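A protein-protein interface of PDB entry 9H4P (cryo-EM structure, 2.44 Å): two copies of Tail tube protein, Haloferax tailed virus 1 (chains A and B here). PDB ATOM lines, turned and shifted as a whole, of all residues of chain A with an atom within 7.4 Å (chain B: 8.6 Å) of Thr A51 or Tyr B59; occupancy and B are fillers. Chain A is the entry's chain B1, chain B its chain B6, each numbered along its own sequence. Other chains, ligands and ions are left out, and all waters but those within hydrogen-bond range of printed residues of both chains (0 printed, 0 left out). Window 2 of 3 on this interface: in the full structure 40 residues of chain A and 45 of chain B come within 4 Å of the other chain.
The backbone carbonyl oxygen (O) of Ala B39 sits at hydrogen-bond distance from a ring nitrogen (ND1) of His B61 (2.8 Å).
O of Glu B41 lies within hydrogen-bond range of N of Tyr B59 (2.8 Å).
The backbone carbonyl oxygen of Glu B60 is in hydrogen-bond range of the backbone NH of Glu B41 (3.1 Å).
The side-chain hydroxyl (OG) of Ser A50 is in hydrogen-bond range of the backbone NH (N) of Phe A52 (3.0 Å).
NE of Arg B147 sits at hydrogen-bond distance from O of Arg A53.
N of His B61 lies within hydrogen-bond range of O of Thr A51 (2.9 Å).
The side-chain hydroxyl (OH) of Tyr A46 sits at hydrogen-bond distance from the backbone carbonyl oxygen (O) of His B61, 2.8 Å away.
Thr A51 touches just these residues of chain B: Tyr B59, Glu B60 and His B61.
Of chain A, only Thr A51 comes within 4 Å of Tyr B59.
Of the printed residues of chain A, His B61 touches Tyr A46, Thr A51 and Phe A52.
Of the printed residues of chain A, Glu B60 touches Tyr A46 and Thr A51.
Of the printed residues of chain B, Arg A53 touches Arg B147 (2.8 Å).
The nearest residue of chain A that does not touch Tyr B59 is Phe A52 (5.6 Å).
Among the printed residues, pairs that only touch across the chains: Tyr A46 with Glu B60 (3.8 Å), Thr A51 with Tyr B59 (3.2 Å), Thr A51 with Glu B60 (3.8 Å), Phe A52 with His B61 (3.5 Å) and Phe A52 with Arg B147 (3.7 Å).
Of the 9 printed residues of chain A, 4 touch a printed residue of chain B.
Printed residues of chain A that touch a printed residue of chain B: Tyr A46, Thr A51, Phe A52 and Arg A53.
Hydrophobic or aromatic side chains of chain A within 4 Å of the printed part of chain B: Tyr A46 and Phe A52.
Of the 16 printed residues of chain B, 4 touch a printed residue of chain A.
Hydrophobic or aromatic side chains of chain B that line the printed part of chain A: His B61.
Among the printed residues, no Asp or Glu carboxylate lies within 4 Å of a Lys or Arg side-chain nitrogen of the other chain.
No position is printed for both chains.
Of the 8 pairs that touch across the chains among the printed residues, none has its exchanged pair printed and touching as well.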
ATOM      1  N   TYR A  46     -24.252  -2.268 -26.920  1.00  0.00           N
ATOM      2  CA  TYR A  46     -23.007  -2.674 -26.270  1.00  0.00           C
ATOM      3  C   TYR A  46     -21.958  -1.557 -26.398  1.00  0.00           C
ATOM      4  O   TYR A  46     -22.050  -0.738 -27.316  1.00  0.00           O
ATOM      5  CB  TYR A  46     -22.532  -4.010 -26.865  1.00  0.00           C
ATOM      6  CG  TYR A  46     -23.436  -5.197 -26.611  1.00  0.00           C
ATOM      7  CD1 TYR A  46     -24.573  -5.433 -27.383  1.00  0.00           C
ATOM      8  CD2 TYR A  46     -23.153  -6.095 -25.588  1.00  0.00           C
ATOM      9  CE1 TYR A  46     -25.409  -6.516 -27.132  1.00  0.00           C
ATOM     10  CE2 TYR A  46     -23.975  -7.186 -25.330  1.00  0.00           C
ATOM     11  CZ  TYR A  46     -25.110  -7.396 -26.101  1.00  0.00           C
ATOM     12  OH  TYR A  46     -25.913  -8.474 -25.851  1.00  0.00           O
ATOM     13  N   THR A  47     -20.960  -1.523 -25.488  1.00  0.00           N
ATOM     14  CA  THR A  47     -19.841  -0.575 -25.542  1.00  0.00           C
ATOM     15  C   THR A  47     -18.628  -1.221 -26.230  1.00  0.00           C
ATOM     16  O   THR A  47     -18.675  -2.405 -26.569  1.00  0.00           O
ATOM     17  CB  THR A  47     -19.433  -0.051 -24.150  1.00  0.00           C
ATOM     18  OG1 THR A  47     -18.607  -1.005 -23.481  1.00  0.00           O
ATOM     19  CG2 THR A  47     -20.590   0.291 -23.241  1.00  0.00           C
ATOM     20  N   ILE A  48     -17.518  -0.468 -26.364  1.00  0.00           N
ATOM     21  CA  ILE A  48     -16.301  -0.905 -27.054  1.00  0.00           C
ATOM     22  C   ILE A  48     -15.433  -1.881 -26.245  1.00  0.00           C
ATOM     23  O   ILE A  48     -14.542  -2.500 -26.828  1.00  0.00           O
ATOM     24  CB  ILE A  48     -15.439   0.295 -27.527  1.00  0.00           C
ATOM     25  CG1 ILE A  48     -15.065   1.261 -26.390  1.00  0.00           C
ATOM     26  CG2 ILE A  48     -16.074   1.006 -28.715  1.00  0.00           C
ATOM     27  CD1 ILE A  48     -14.069   2.347 -26.768  1.00  0.00           C
ATOM     28  N   ASP A  49     -15.653  -2.001 -24.923  1.00  0.00           N
ATOM     29  CA  ASP A  49     -14.678  -2.644 -24.044  1.00  0.00           C
ATOM     30  C   ASP A  49     -15.351  -3.606 -23.059  1.00  0.00           C
ATOM     31  O   ASP A  49     -14.830  -3.848 -21.967  1.00  0.00           O
ATOM     32  CB  ASP A  49     -13.787  -1.595 -23.355  1.00  0.00           C
ATOM     33  CG  ASP A  49     -12.504  -2.129 -22.730  1.00  0.00           C
ATOM     34  OD1 ASP A  49     -12.022  -3.192 -23.170  1.00  0.00           O
ATOM     35  OD2 ASP A  49     -11.990  -1.469 -21.807  1.00  0.00           O
ATOM     36  N   SER A  50     -16.498  -4.171 -23.459  1.00  0.00           N
ATOM     37  CA  SER A  50     -17.254  -5.080 -22.610  1.00  0.00           C
ATOM     38  C   SER A  50     -18.087  -6.028 -23.473  1.00  0.00           C
ATOM     39  O   SER A  50     -18.647  -5.616 -24.490  1.00  0.00           O
ATOM     40  CB  SER A  50     -18.128  -4.306 -21.638  1.00  0.00           C
ATOM     41  OG  SER A  50     -18.948  -5.169 -20.862  1.00  0.00           O
ATOM     42  N   THR A  51     -18.182  -7.285 -23.021  1.00  0.00           N
ATOM     43  CA  THR A  51     -19.096  -8.277 -23.575  1.00  0.00           C
ATOM     44  C   THR A  51     -20.532  -8.036 -23.099  1.00  0.00           C
ATOM     45  O   THR A  51     -21.471  -8.548 -23.710  1.00  0.00           O
ATOM     46  CB  THR A  51     -18.683  -9.709 -23.196  1.00  0.00           C
ATOM     47  OG1 THR A  51     -18.717  -9.880 -21.777  1.00  0.00           O
ATOM     48  CG2 THR A  51     -17.320 -10.106 -23.727  1.00  0.00           C
ATOM     49  N   PHE A  52     -20.705  -7.271 -22.009  1.00  0.00           N
ATOM     50  CA  PHE A  52     -22.017  -7.096 -21.394  1.00  0.00           C
ATOM     51  C   PHE A  52     -22.791  -5.956 -22.063  1.00  0.00           C
ATOM     52  O   PHE A  52     -22.199  -4.977 -22.525  1.00  0.00           O
ATOM     53  CB  PHE A  52     -21.894  -6.849 -19.885  1.00  0.00           C
ATOM     54  CG  PHE A  52     -21.443  -8.001 -19.015  1.00  0.00           C
ATOM     55  CD1 PHE A  52     -21.164  -9.269 -19.528  1.00  0.00           C
ATOM     56  CD2 PHE A  52     -21.334  -7.807 -17.643  1.00  0.00           C
ATOM     57  CE1 PHE A  52     -20.765 -10.300 -18.686  1.00  0.00           C
ATOM     58  CE2 PHE A  52     -20.942  -8.840 -16.800  1.00  0.00           C
ATOM     59  CZ  PHE A  52     -20.655 -10.085 -17.325  1.00  0.00           C
ATOM     60  N   ARG A  53     -24.123  -6.113 -22.089  1.00  0.00           N
ATOM     61  CA  ARG A  53     -25.076  -5.145 -22.617  1.00  0.00           C
ATOM     62  C   ARG A  53     -25.003  -3.844 -21.809  1.00  0.00           C
ATOM     63  O   ARG A  53     -25.030  -3.874 -20.576  1.00  0.00           O
ATOM     64  CB  ARG A  53     -26.470  -5.784 -22.562  1.00  0.00           C
ATOM     65  CG  ARG A  53     -27.550  -5.073 -23.366  1.00  0.00           C
ATOM     66  CD  ARG A  53     -28.868  -5.819 -23.221  1.00  0.00           C
ATOM     67  NE  ARG A  53     -29.461  -5.663 -21.891  1.00  0.00           N
ATOM     68  CZ  ARG A  53     -30.407  -6.432 -21.340  1.00  0.00           C
ATOM     69  NH1 ARG A  53     -30.844  -6.154 -20.122  1.00  0.00           N
ATOM     70  NH2 ARG A  53     -30.917  -7.466 -21.992  1.00  0.00           N
ATOM     71  N   ASP A  54     -24.925  -2.708 -22.519  1.00  0.00           N
ATOM     72  CA  ASP A  54     -24.829  -1.388 -21.908  1.00  0.00           C
ATOM     73  C   ASP A  54     -26.227  -0.852 -21.596  1.00  0.00           C
ATOM     74  O   ASP A  54     -26.507  -0.449 -20.464  1.00  0.00           O
ATOM     75  CB  ASP A  54     -24.050  -0.422 -22.807  1.00  0.00           C
ATOM     76  CG  ASP A  54     -23.748   0.919 -22.155  1.00  0.00           C
ATOM     77  OD1 ASP A  54     -23.562   0.949 -20.921  1.00  0.00           O
ATOM     78  OD2 ASP A  54     -23.686   1.918 -22.890  1.00  0.00           O
ATOM     79  N   ALA B  39     -25.652 -17.017 -22.511  1.00  0.00           N
ATOM     80  CA  ALA B  39     -25.126 -17.250 -23.844  1.00  0.00           C
ATOM     81  C   ALA B  39     -24.096 -16.173 -24.179  1.00  0.00           C
ATOM     82  O   ALA B  39     -24.120 -15.077 -23.617  1.00  0.00           O
ATOM     83  CB  ALA B  39     -26.262 -17.246 -24.845  1.00  0.00           C
ATOM     84  N   TYR B  40     -23.201 -16.510 -25.111  1.00  0.00           N
ATOM     85  CA  TYR B  40     -22.354 -15.533 -25.775  1.00  0.00           C
ATOM     86  C   TYR B  40     -22.332 -15.876 -27.265  1.00  0.00           C
ATOM     87  O   TYR B  40     -22.431 -17.052 -27.632  1.00  0.00           O
ATOM     88  CB  TYR B  40     -20.913 -15.611 -25.253  1.00  0.00           C
ATOM     89  CG  TYR B  40     -20.638 -15.298 -23.797  1.00  0.00           C
ATOM     90  CD1 TYR B  40     -20.896 -16.223 -22.785  1.00  0.00           C
ATOM     91  CD2 TYR B  40     -20.012 -14.106 -23.442  1.00  0.00           C
ATOM     92  CE1 TYR B  40     -20.592 -15.943 -21.457  1.00  0.00           C
ATOM     93  CE2 TYR B  40     -19.698 -13.813 -22.119  1.00  0.00           C
ATOM     94  CZ  TYR B  40     -19.990 -14.735 -21.122  1.00  0.00           C
ATOM     95  OH  TYR B  40     -19.698 -14.458 -19.815  1.00  0.00           O
ATOM     96  N   GLU B  41     -22.192 -14.850 -28.114  1.00  0.00           N
ATOM     97  CA  GLU B  41     -21.725 -15.091 -29.471  1.00  0.00           C
ATOM     98  C   GLU B  41     -20.293 -15.629 -29.398  1.00  0.00           C
ATOM     99  O   GLU B  41     -19.455 -15.059 -28.695  1.00  0.00           O
ATOM    100  CB  GLU B  41     -21.767 -13.800 -30.296  1.00  0.00           C
ATOM    101  CG  GLU B  41     -23.162 -13.237 -30.519  1.00  0.00           C
ATOM    102  CD  GLU B  41     -24.165 -14.201 -31.129  1.00  0.00           C
ATOM    103  OE1 GLU B  41     -23.772 -15.016 -31.989  1.00  0.00           O
ATOM    104  OE2 GLU B  41     -25.341 -14.134 -30.738  1.00  0.00           O
ATOM    105  N   HIS B  42     -20.035 -16.746 -30.096  1.00  0.00           N
ATOM    106  CA  HIS B  42     -18.683 -17.270 -30.252  1.00  0.00           C
ATOM    107  C   HIS B  42     -18.181 -16.941 -31.656  1.00  0.00           C
ATOM    108  O   HIS B  42     -18.799 -17.348 -32.642  1.00  0.00           O
ATOM    109  CB  HIS B  42     -18.633 -18.790 -29.992  1.00  0.00           C
ATOM    110  CG  HIS B  42     -18.630 -19.176 -28.548  1.00  0.00           C
ATOM    111  ND1 HIS B  42     -18.282 -20.447 -28.110  1.00  0.00           N
ATOM    112  CD2 HIS B  42     -18.925 -18.462 -27.439  1.00  0.00           C
ATOM    113  CE1 HIS B  42     -18.369 -20.496 -26.794  1.00  0.00           C
ATOM    114  NE2 HIS B  42     -18.763 -19.287 -26.358  1.00  0.00           N
ATOM    115  N   ALA B  43     -17.079 -16.184 -31.733  1.00  0.00           N
ATOM    116  CA  ALA B  43     -16.307 -16.068 -32.962  1.00  0.00           C
ATOM    117  C   ALA B  43     -15.372 -17.274 -33.061  1.00  0.00           C
ATOM    118  O   ALA B  43     -14.465 -17.414 -32.237  1.00  0.00           O
ATOM    119  CB  ALA B  43     -15.550 -14.758 -32.969  1.00  0.00           C
ATOM    120  N   GLU B  44     -15.603 -18.137 -34.067  1.00  0.00           N
ATOM    121  CA  GLU B  44     -14.936 -19.429 -34.185  1.00  0.00           C
ATOM    122  C   GLU B  44     -13.895 -19.352 -35.309  1.00  0.00           C
ATOM    123  O   GLU B  44     -14.257 -19.366 -36.486  1.00  0.00           O
ATOM    124  CB  GLU B  44     -15.996 -20.521 -34.376  1.00  0.00           C
ATOM    125  CG  GLU B  44     -15.481 -21.911 -34.067  1.00  0.00           C
ATOM    126  CD  GLU B  44     -16.505 -23.022 -33.965  1.00  0.00           C
ATOM    127  OE1 GLU B  44     -17.641 -22.839 -34.442  1.00  0.00           O
ATOM    128  OE2 GLU B  44     -16.156 -24.073 -33.415  1.00  0.00           O
ATOM    129  N   LEU B  45     -12.602 -19.271 -34.939  1.00  0.00           N
ATOM    130  CA  LEU B  45     -11.580 -18.653 -35.784  1.00  0.00           C
ATOM    131  C   LEU B  45     -10.611 -19.680 -36.385  1.00  0.00           C
ATOM    132  O   LEU B  45     -10.118 -20.557 -35.672  1.00  0.00           O
ATOM    133  CB  LEU B  45     -10.811 -17.600 -34.968  1.00  0.00           C
ATOM    134  CG  LEU B  45     -11.640 -16.502 -34.288  1.00  0.00           C
ATOM    135  CD1 LEU B  45     -10.802 -15.730 -33.276  1.00  0.00           C
ATOM    136  CD2 LEU B  45     -12.261 -15.546 -35.304  1.00  0.00           C
ATOM    137  N   VAL B  56     -11.117 -19.643 -30.404  1.00  0.00           N
ATOM    138  CA  VAL B  56     -12.517 -19.247 -30.291  1.00  0.00           C
ATOM    139  C   VAL B  56     -12.656 -18.197 -29.183  1.00  0.00           C
ATOM    140  O   VAL B  56     -12.041 -18.327 -28.121  1.00  0.00           O
ATOM    141  CB  VAL B  56     -13.458 -20.466 -30.128  1.00  0.00           C
ATOM    142  CG1 VAL B  56     -13.038 -21.423 -29.012  1.00  0.00           C
ATOM    143  CG2 VAL B  56     -14.937 -20.094 -30.026  1.00  0.00           C
ATOM    144  N   LYS B  57     -13.464 -17.155 -29.452  1.00  0.00           N
ATOM    145  CA  LYS B  57     -13.586 -15.979 -28.597  1.00  0.00           C
ATOM    146  C   LYS B  57     -15.061 -15.657 -28.336  1.00  0.00           C
ATOM    147  O   LYS B  57     -15.880 -15.717 -29.255  1.00  0.00           O
ATOM    148  CB  LYS B  57     -12.876 -14.769 -29.226  1.00  0.00           C
ATOM    149  CG  LYS B  57     -11.354 -14.853 -29.315  1.00  0.00           C
ATOM    150  CD  LYS B  57     -10.652 -14.713 -27.975  1.00  0.00           C
ATOM    151  CE  LYS B  57      -9.153 -14.900 -28.084  1.00  0.00           C
ATOM    152  NZ  LYS B  57      -8.463 -14.627 -26.803  1.00  0.00           N
ATOM    153  N   ARG B  58     -15.383 -15.295 -27.083  1.00  0.00           N
ATOM    154  CA  ARG B  58     -16.710 -14.817 -26.706  1.00  0.00           C
ATOM    155  C   ARG B  58     -16.839 -13.336 -27.064  1.00  0.00           C
ATOM    156  O   ARG B  58     -15.874 -12.582 -26.916  1.00  0.00           O
ATOM    157  CB  ARG B  58     -16.942 -14.966 -25.196  1.00  0.00           C
ATOM    158  CG  ARG B  58     -16.676 -16.365 -24.656  1.00  0.00           C
ATOM    159  CD  ARG B  58     -17.316 -16.657 -23.308  1.00  0.00           C
ATOM    160  NE  ARG B  58     -16.610 -16.113 -22.148  1.00  0.00           N
ATOM    161  CZ  ARG B  58     -16.706 -16.585 -20.904  1.00  0.00           C
ATOM    162  NH1 ARG B  58     -16.024 -16.015 -19.927  1.00  0.00           N
ATOM    163  NH2 ARG B  58     -17.474 -17.629 -20.638  1.00  0.00           N
ATOM    164  N   TYR B  59     -18.033 -12.929 -27.532  1.00  0.00           N
ATOM    165  CA  TYR B  59     -18.383 -11.512 -27.605  1.00  0.00           C
ATOM    166  C   TYR B  59     -19.726 -11.219 -26.921  1.00  0.00           C
ATOM    167  O   TYR B  59     -19.809 -11.377 -25.700  1.00  0.00           O
ATOM    168  CB  TYR B  59     -18.026 -10.847 -28.943  1.00  0.00           C
ATOM    169  CG  TYR B  59     -18.660 -11.359 -30.216  1.00  0.00           C
ATOM    170  CD1 TYR B  59     -18.189 -12.508 -30.846  1.00  0.00           C
ATOM    171  CD2 TYR B  59     -19.671 -10.639 -30.846  1.00  0.00           C
ATOM    172  CE1 TYR B  59     -18.740 -12.958 -32.040  1.00  0.00           C
ATOM    173  CE2 TYR B  59     -20.229 -11.073 -32.041  1.00  0.00           C
ATOM    174  CZ  TYR B  59     -19.760 -12.234 -32.639  1.00  0.00           C
ATOM    175  OH  TYR B  59     -20.318 -12.666 -33.807  1.00  0.00           O
ATOM    176  N   GLU B  60     -20.758 -10.800 -27.678  1.00  0.00           N
ATOM    177  CA  GLU B  60     -21.977 -10.248 -27.092  1.00  0.00           C
ATOM    178  C   GLU B  60     -22.631 -11.248 -26.131  1.00  0.00           C
ATOM    179  O   GLU B  60     -23.069 -12.322 -26.553  1.00  0.00           O
ATOM    180  CB  GLU B  60     -22.959  -9.802 -28.181  1.00  0.00           C
ATOM    181  CG  GLU B  60     -22.531  -8.548 -28.927  1.00  0.00           C
ATOM    182  CD  GLU B  60     -23.148  -8.413 -30.306  1.00  0.00           C
ATOM    183  OE1 GLU B  60     -24.355  -8.695 -30.450  1.00  0.00           O
ATOM    184  OE2 GLU B  60     -22.419  -8.030 -31.235  1.00  0.00           O
ATOM    185  N   HIS B  61     -22.688 -10.869 -24.840  1.00  0.00           N
ATOM    186  CA  HIS B  61     -23.293 -11.673 -23.782  1.00  0.00           C
ATOM    187  C   HIS B  61     -24.751 -11.262 -23.556  1.00  0.00           C
ATOM    188  O   HIS B  61     -25.098 -10.084 -23.693  1.00  0.00           O
ATOM    189  CB  HIS B  61     -22.465 -11.561 -22.483  1.00  0.00           C
ATOM    190  CG  HIS B  61     -23.002 -12.354 -21.331  1.00  0.00           C
ATOM    191  ND1 HIS B  61     -23.109 -13.740 -21.364  1.00  0.00           N
ATOM    192  CD2 HIS B  61     -23.452 -11.969 -20.114  1.00  0.00           C
ATOM    193  CE1 HIS B  61     -23.610 -14.172 -20.222  1.00  0.00           C
ATOM    194  NE2 HIS B  61     -23.834 -13.101 -19.440  1.00  0.00           N
ATOM    195  N   ASN B  62     -25.585 -12.254 -23.201  1.00  0.00           N
ATOM    196  CA  ASN B  62     -26.945 -12.060 -22.713  1.00  0.00           C
ATOM    197  C   ASN B  62     -27.379 -13.328 -21.972  1.00  0.00           C
ATOM    198  O   ASN B  62     -26.744 -14.378 -22.108  1.00  0.00           O
ATOM    199  CB  ASN B  62     -27.927 -11.720 -23.847  1.00  0.00           C
ATOM    200  CG  ASN B  62     -28.192 -12.879 -24.793  1.00  0.00           C
ATOM    201  OD1 ASN B  62     -27.263 -13.516 -25.291  1.00  0.00           O
ATOM    202  ND2 ASN B  62     -29.459 -13.161 -25.054  1.00  0.00           N
ATOM    203  N   ARG B 147     -29.142  -9.149 -18.583  1.00  0.00           N
ATOM    204  CA  ARG B 147     -27.808  -8.636 -18.868  1.00  0.00           C
ATOM    205  C   ARG B 147     -26.733  -9.673 -18.520  1.00  0.00           C
ATOM    206  O   ARG B 147     -25.811  -9.885 -19.314  1.00  0.00           O
ATOM    207  CB  ARG B 147     -27.592  -7.297 -18.156  1.00  0.00           C
ATOM    208  CG  ARG B 147     -26.206  -6.705 -18.369  1.00  0.00           C
ATOM    209  CD  ARG B 147     -26.100  -5.349 -17.697  1.00  0.00           C
ATOM    210  NE  ARG B 147     -24.792  -4.727 -17.874  1.00  0.00           N
ATOM    211  CZ  ARG B 147     -23.738  -4.866 -17.064  1.00  0.00           C
ATOM    212  NH1 ARG B 147     -22.613  -4.229 -17.343  1.00  0.00           N
ATOM    213  NH2 ARG B 147     -23.801  -5.631 -15.986  1.00  0.00           N
ATOM    214  N   SER B 148     -26.856 -10.300 -17.334  1.00  0.00           N
ATOM    215  CA  SER B 148     -25.887 -11.276 -16.839  1.00  0.00           C
ATOM    216  C   SER B 148     -26.500 -12.143 -15.734  1.00  0.00           C
ATOM    217  O   SER B 148     -27.531 -11.787 -15.158  1.00  0.00           O
ATOM    218  CB  SER B 148     -24.599 -10.599 -16.374  1.00  0.00           C
ATOM    219  OG  SER B 148     -24.784  -9.899 -15.150  1.00  0.00           O
